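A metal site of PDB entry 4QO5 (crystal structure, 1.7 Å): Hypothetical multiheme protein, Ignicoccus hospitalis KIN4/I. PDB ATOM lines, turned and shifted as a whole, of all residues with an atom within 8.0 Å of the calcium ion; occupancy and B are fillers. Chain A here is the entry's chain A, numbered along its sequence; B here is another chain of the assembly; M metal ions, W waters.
The calcium ion is bound by the backbone carbonyl oxygen (O) of Thr 459, the backbone carbonyl oxygen (O) of His 451, the side-chain carboxylate (OE2) of Glu 466, water W1, the side-chain carboxylate (OD1) of Asp 462, the side-chain carboxylate (OE2) of Glu 463 and the side-chain carboxylate (OE1) of Glu 466. The calcium ion has seven donor atoms within binding distance.
OG1 of Thr 459 sits at hydrogen-bond distance from N of Asp 453 (2.9 Å). O of Lys 456 sits at hydrogen-bond distance from OG1 of Thr 459. The side-chain carboxylate of Glu 466 sits close to the indole nitrogen of Trp 445.
Of the 19 residues printed, 5 come within 4 Å of the calcium ion.
Water W1 bridges OD2 of Asp 462 and ND1 of His 451.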
ATOM      1  N   LEU A 441      -1.408 -15.814  28.777  1.00  0.00           N
ATOM      2  CA  LEU A 441      -0.723 -16.535  27.707  1.00  0.00           C
ATOM      3  C   LEU A 441       0.193 -15.602  26.893  1.00  0.00           C
ATOM      4  O   LEU A 441       1.306 -15.988  26.541  1.00  0.00           O
ATOM      5  CB  LEU A 441      -1.703 -17.252  26.793  1.00  0.00           C
ATOM      6  CG  LEU A 441      -0.995 -18.127  25.746  1.00  0.00           C
ATOM      7  CD1 LEU A 441       0.001 -19.096  26.387  1.00  0.00           C
ATOM      8  CD2 LEU A 441      -2.012 -18.900  24.953  1.00  0.00           C
ATOM      9  N   TRP A 445       4.234 -16.034  26.257  1.00  0.00           N
ATOM     10  CA  TRP A 445       4.923 -15.963  24.984  1.00  0.00           C
ATOM     11  C   TRP A 445       5.978 -14.854  25.003  1.00  0.00           C
ATOM     12  O   TRP A 445       7.079 -15.020  24.488  1.00  0.00           O
ATOM     13  CB  TRP A 445       3.934 -15.732  23.844  1.00  0.00           C
ATOM     14  CG  TRP A 445       3.091 -16.906  23.497  1.00  0.00           C
ATOM     15  CD1 TRP A 445       3.409 -18.232  23.672  1.00  0.00           C
ATOM     16  CD2 TRP A 445       1.787 -16.881  22.911  1.00  0.00           C
ATOM     17  NE1 TRP A 445       2.379 -19.018  23.223  1.00  0.00           N
ATOM     18  CE2 TRP A 445       1.376 -18.212  22.756  1.00  0.00           C
ATOM     19  CE3 TRP A 445       0.938 -15.840  22.506  1.00  0.00           C
ATOM     20  CZ2 TRP A 445       0.133 -18.543  22.217  1.00  0.00           C
ATOM     21  CZ3 TRP A 445      -0.300 -16.179  21.966  1.00  0.00           C
ATOM     22  CH2 TRP A 445      -0.690 -17.514  21.830  1.00  0.00           C
ATOM     23  N   LEU A 449       8.500 -18.411  28.123  1.00  0.00           N
ATOM     24  CA  LEU A 449       8.100 -19.645  28.788  1.00  0.00           C
ATOM     25  C   LEU A 449       7.463 -20.581  27.760  1.00  0.00           C
ATOM     26  O   LEU A 449       7.549 -21.807  27.894  1.00  0.00           O
ATOM     27  CB  LEU A 449       7.130 -19.362  29.933  1.00  0.00           C
ATOM     28  CG  LEU A 449       6.508 -20.554  30.658  1.00  0.00           C
ATOM     29  CD1 LEU A 449       7.570 -21.487  31.234  1.00  0.00           C
ATOM     30  CD2 LEU A 449       5.572 -20.070  31.758  1.00  0.00           C
ATOM     31  N   ALA A 450       6.833 -20.000  26.742  1.00  0.00           N
ATOM     32  CA  ALA A 450       6.227 -20.771  25.662  1.00  0.00           C
ATOM     33  C   ALA A 450       6.566 -20.140  24.320  1.00  0.00           C
ATOM     34  O   ALA A 450       6.871 -18.953  24.248  1.00  0.00           O
ATOM     35  CB  ALA A 450       4.722 -20.858  25.841  1.00  0.00           C
ATOM     36  N   HIS A 451       6.503 -20.953  23.270  1.00  0.00           N
ATOM     37  CA  HIS A 451       6.867 -20.536  21.909  1.00  0.00           C
ATOM     38  C   HIS A 451       5.631 -20.419  21.035  1.00  0.00           C
ATOM     39  O   HIS A 451       4.710 -21.224  21.141  1.00  0.00           O
ATOM     40  CB  HIS A 451       7.849 -21.547  21.293  1.00  0.00           C
ATOM     41  CG  HIS A 451       7.952 -21.470  19.802  1.00  0.00           C
ATOM     42  ND1 HIS A 451       7.304 -22.353  18.957  1.00  0.00           N
ATOM     43  CD2 HIS A 451       8.633 -20.610  18.997  1.00  0.00           C
ATOM     44  CE1 HIS A 451       7.578 -22.039  17.701  1.00  0.00           C
ATOM     45  NE2 HIS A 451       8.376 -20.997  17.689  1.00  0.00           N
ATOM     46  N   VAL A 452       5.611 -19.445  20.144  1.00  0.00           N
ATOM     47  CA  VAL A 452       4.481 -19.289  19.246  1.00  0.00           C
ATOM     48  C   VAL A 452       4.956 -18.841  17.860  1.00  0.00           C
ATOM     49  O   VAL A 452       5.938 -18.105  17.741  1.00  0.00           O
ATOM     50  CB  VAL A 452       3.411 -18.318  19.815  1.00  0.00           C
ATOM     51  CG1 VAL A 452       3.917 -16.879  19.796  1.00  0.00           C
ATOM     52  CG2 VAL A 452       2.103 -18.450  19.069  1.00  0.00           C
ATOM     53  N   ASP A 453       4.264 -19.309  16.825  1.00  0.00           N
ATOM     54  CA  ASP A 453       4.569 -18.988  15.428  1.00  0.00           C
ATOM     55  C   ASP A 453       3.265 -19.099  14.645  1.00  0.00           C
ATOM     56  O   ASP A 453       2.796 -20.199  14.379  1.00  0.00           O
ATOM     57  CB  ASP A 453       5.625 -19.960  14.889  1.00  0.00           C
ATOM     58  CG  ASP A 453       5.864 -19.817  13.389  1.00  0.00           C
ATOM     59  OD1 ASP A 453       5.449 -18.812  12.781  1.00  0.00           O
ATOM     60  OD2 ASP A 453       6.507 -20.731  12.803  1.00  0.00           O
ATOM     61  N   LYS A 456       2.469 -21.372  11.803  1.00  0.00           N
ATOM     62  CA  LYS A 456       2.342 -22.772  12.181  1.00  0.00           C
ATOM     63  C   LYS A 456       1.447 -22.856  13.412  1.00  0.00           C
ATOM     64  O   LYS A 456       1.945 -22.974  14.536  1.00  0.00           O
ATOM     65  CB  LYS A 456       3.705 -23.357  12.523  1.00  0.00           C
ATOM     66  CG  LYS A 456       4.442 -24.035  11.379  1.00  0.00           C
ATOM     67  CD  LYS A 456       4.689 -25.510  11.711  1.00  0.00           C
ATOM     68  CE  LYS A 456       5.493 -25.674  12.996  1.00  0.00           C
ATOM     69  NZ  LYS A 456       5.451 -27.069  13.537  1.00  0.00           N
ATOM     70  N   PRO A 457       0.121 -22.811  13.217  1.00  0.00           N
ATOM     71  CA  PRO A 457      -0.883 -22.706  14.290  1.00  0.00           C
ATOM     72  C   PRO A 457      -0.839 -23.837  15.346  1.00  0.00           C
ATOM     73  O   PRO A 457      -1.377 -23.652  16.440  1.00  0.00           O
ATOM     74  CB  PRO A 457      -2.221 -22.740  13.552  1.00  0.00           C
ATOM     75  CG  PRO A 457      -1.911 -22.448  12.139  1.00  0.00           C
ATOM     76  CD  PRO A 457      -0.514 -22.892  11.886  1.00  0.00           C
ATOM     77  N   VAL A 458      -0.229 -24.971  15.045  1.00  0.00           N
ATOM     78  CA  VAL A 458      -0.134 -26.019  16.055  1.00  0.00           C
ATOM     79  C   VAL A 458       0.651 -25.499  17.271  1.00  0.00           C
ATOM     80  O   VAL A 458       0.458 -25.963  18.398  1.00  0.00           O
ATOM     81  CB  VAL A 458       0.495 -27.315  15.491  1.00  0.00           C
ATOM     82  CG1 VAL A 458       1.968 -27.100  15.153  1.00  0.00           C
ATOM     83  CG2 VAL A 458       0.343 -28.472  16.483  1.00  0.00           C
ATOM     84  N   THR A 459       1.522 -24.515  17.045  1.00  0.00           N
ATOM     85  CA  THR A 459       2.345 -23.932  18.099  1.00  0.00           C
ATOM     86  C   THR A 459       1.557 -23.093  19.100  1.00  0.00           C
ATOM     87  O   THR A 459       2.103 -22.644  20.112  1.00  0.00           O
ATOM     88  CB  THR A 459       3.473 -23.054  17.528  1.00  0.00           C
ATOM     89  OG1 THR A 459       2.906 -21.904  16.866  1.00  0.00           O
ATOM     90  CG2 THR A 459       4.313 -23.845  16.546  1.00  0.00           C
ATOM     91  N   LEU A 460       0.278 -22.864  18.805  1.00  0.00           N
ATOM     92  CA  LEU A 460      -0.603 -22.156  19.732  1.00  0.00           C
ATOM     93  C   LEU A 460      -1.001 -23.051  20.885  1.00  0.00           C
ATOM     94  O   LEU A 460      -1.388 -22.546  21.944  1.00  0.00           O
ATOM     95  CB  LEU A 460      -1.860 -21.688  19.023  1.00  0.00           C
ATOM     96  CG  LEU A 460      -1.687 -20.619  17.944  1.00  0.00           C
ATOM     97  CD1 LEU A 460      -2.916 -20.555  17.061  1.00  0.00           C
ATOM     98  CD2 LEU A 460      -1.431 -19.275  18.632  1.00  0.00           C
ATOM     99  N   PHE A 461      -0.926 -24.372  20.686  1.00  0.00           N
ATOM    100  CA  PHE A 461      -1.608 -25.323  21.546  1.00  0.00           C
ATOM    101  C   PHE A 461      -0.723 -26.479  21.992  1.00  0.00           C
ATOM    102  O   PHE A 461      -1.231 -27.452  22.552  1.00  0.00           O
ATOM    103  CB  PHE A 461      -2.815 -25.947  20.823  1.00  0.00           C
ATOM    104  CG  PHE A 461      -3.748 -24.948  20.207  1.00  0.00           C
ATOM    105  CD1 PHE A 461      -4.470 -24.070  21.001  1.00  0.00           C
ATOM    106  CD2 PHE A 461      -3.939 -24.915  18.833  1.00  0.00           C
ATOM    107  CE1 PHE A 461      -5.347 -23.166  20.439  1.00  0.00           C
ATOM    108  CE2 PHE A 461      -4.807 -24.027  18.258  1.00  0.00           C
ATOM    109  CZ  PHE A 461      -5.520 -23.145  19.062  1.00  0.00           C
ATOM    110  N   ASP A 462       0.580 -26.388  21.755  1.00  0.00           N
ATOM    111  CA  ASP A 462       1.443 -27.552  21.863  1.00  0.00           C
ATOM    112  C   ASP A 462       2.267 -27.648  23.151  1.00  0.00           C
ATOM    113  O   ASP A 462       2.993 -28.614  23.347  1.00  0.00           O
ATOM    114  CB  ASP A 462       2.350 -27.704  20.630  1.00  0.00           C
ATOM    115  CG  ASP A 462       3.281 -26.520  20.441  1.00  0.00           C
ATOM    116  OD1 ASP A 462       3.182 -25.547  21.206  1.00  0.00           O
ATOM    117  OD2 ASP A 462       4.104 -26.562  19.492  1.00  0.00           O
ATOM    118  N   GLU A 463       2.136 -26.654  24.022  1.00  0.00           N
ATOM    119  CA  GLU A 463       2.868 -26.680  25.282  1.00  0.00           C
ATOM    120  C   GLU A 463       1.936 -26.605  26.481  1.00  0.00           C
ATOM    121  O   GLU A 463       0.778 -26.225  26.355  1.00  0.00           O
ATOM    122  CB  GLU A 463       3.895 -25.546  25.337  1.00  0.00           C
ATOM    123  CG  GLU A 463       4.988 -25.631  24.297  1.00  0.00           C
ATOM    124  CD  GLU A 463       5.786 -24.341  24.199  1.00  0.00           C
ATOM    125  OE1 GLU A 463       6.780 -24.198  24.949  1.00  0.00           O
ATOM    126  OE2 GLU A 463       5.406 -23.476  23.392  1.00  0.00           O
ATOM    127  N   TYR A 464       2.456 -26.983  27.639  1.00  0.00           N
ATOM    128  CA  TYR A 464       1.635 -27.138  28.847  1.00  0.00           C
ATOM    129  C   TYR A 464       0.869 -25.877  29.252  1.00  0.00           C
ATOM    130  O   TYR A 464      -0.337 -25.933  29.465  1.00  0.00           O
ATOM    131  CB  TYR A 464       2.478 -27.675  30.014  1.00  0.00           C
ATOM    132  CG  TYR A 464       1.666 -27.957  31.249  1.00  0.00           C
ATOM    133  CD1 TYR A 464       0.702 -28.964  31.258  1.00  0.00           C
ATOM    134  CD2 TYR A 464       1.835 -27.210  32.409  1.00  0.00           C
ATOM    135  CE1 TYR A 464      -0.052 -29.227  32.374  1.00  0.00           C
ATOM    136  CE2 TYR A 464       1.076 -27.467  33.537  1.00  0.00           C
ATOM    137  CZ  TYR A 464       0.130 -28.481  33.514  1.00  0.00           C
ATOM    138  OH  TYR A 464      -0.615 -28.761  34.627  1.00  0.00           O
ATOM    139  N   ILE A 465       1.546 -24.737  29.361  1.00  0.00           N
ATOM    140  CA  ILE A 465       0.843 -23.508  29.751  1.00  0.00           C
ATOM    141  C   ILE A 465      -0.210 -23.107  28.693  1.00  0.00           C
ATOM    142  O   ILE A 465      -1.232 -22.506  29.032  1.00  0.00           O
ATOM    143  CB  ILE A 465       1.802 -22.331  30.058  1.00  0.00           C
ATOM    144  CG1 ILE A 465       1.032 -21.227  30.801  1.00  0.00           C
ATOM    145  CG2 ILE A 465       2.454 -21.807  28.786  1.00  0.00           C
ATOM    146  CD1 ILE A 465       1.902 -20.205  31.497  1.00  0.00           C
ATOM    147  N   GLU A 466       0.024 -23.463  27.438  1.00  0.00           N
ATOM    148  CA  GLU A 466      -0.936 -23.172  26.380  1.00  0.00           C
ATOM    149  C   GLU A 466      -2.172 -24.057  26.545  1.00  0.00           C
ATOM    150  O   GLU A 466      -3.301 -23.633  26.325  1.00  0.00           O
ATOM    151  CB  GLU A 466      -0.287 -23.370  24.998  1.00  0.00           C
ATOM    152  CG  GLU A 466       0.810 -22.332  24.720  1.00  0.00           C
ATOM    153  CD  GLU A 466       1.802 -22.731  23.635  1.00  0.00           C
ATOM    154  OE1 GLU A 466       1.814 -23.893  23.201  1.00  0.00           O
ATOM    155  OE2 GLU A 466       2.595 -21.849  23.229  1.00  0.00           O
ATOM    156  N   GLU B 506       3.659 -32.949  27.712  1.00  0.00           N
ATOM    157  CA  GLU B 506       4.105 -31.564  27.806  1.00  0.00           C
ATOM    158  C   GLU B 506       4.253 -31.102  29.250  1.00  0.00           C
ATOM    159  O   GLU B 506       5.117 -30.301  29.561  1.00  0.00           O
ATOM    160  CB  GLU B 506       3.160 -30.649  27.044  1.00  0.00           C
ATOM    161  CG  GLU B 506       3.176 -30.920  25.552  1.00  0.00           C
ATOM    162  CD  GLU B 506       4.562 -30.774  24.948  1.00  0.00           C
ATOM    163  OE1 GLU B 506       5.335 -29.915  25.422  1.00  0.00           O
ATOM    164  OE2 GLU B 506       4.872 -31.513  23.989  1.00  0.00           O
HETATM  165 CA    CA M   1       3.678 -23.252  21.657  1.00  0.00          CA
HETATM  166  O   HOH W   1       5.329 -24.093  20.172  1.00  0.00           O
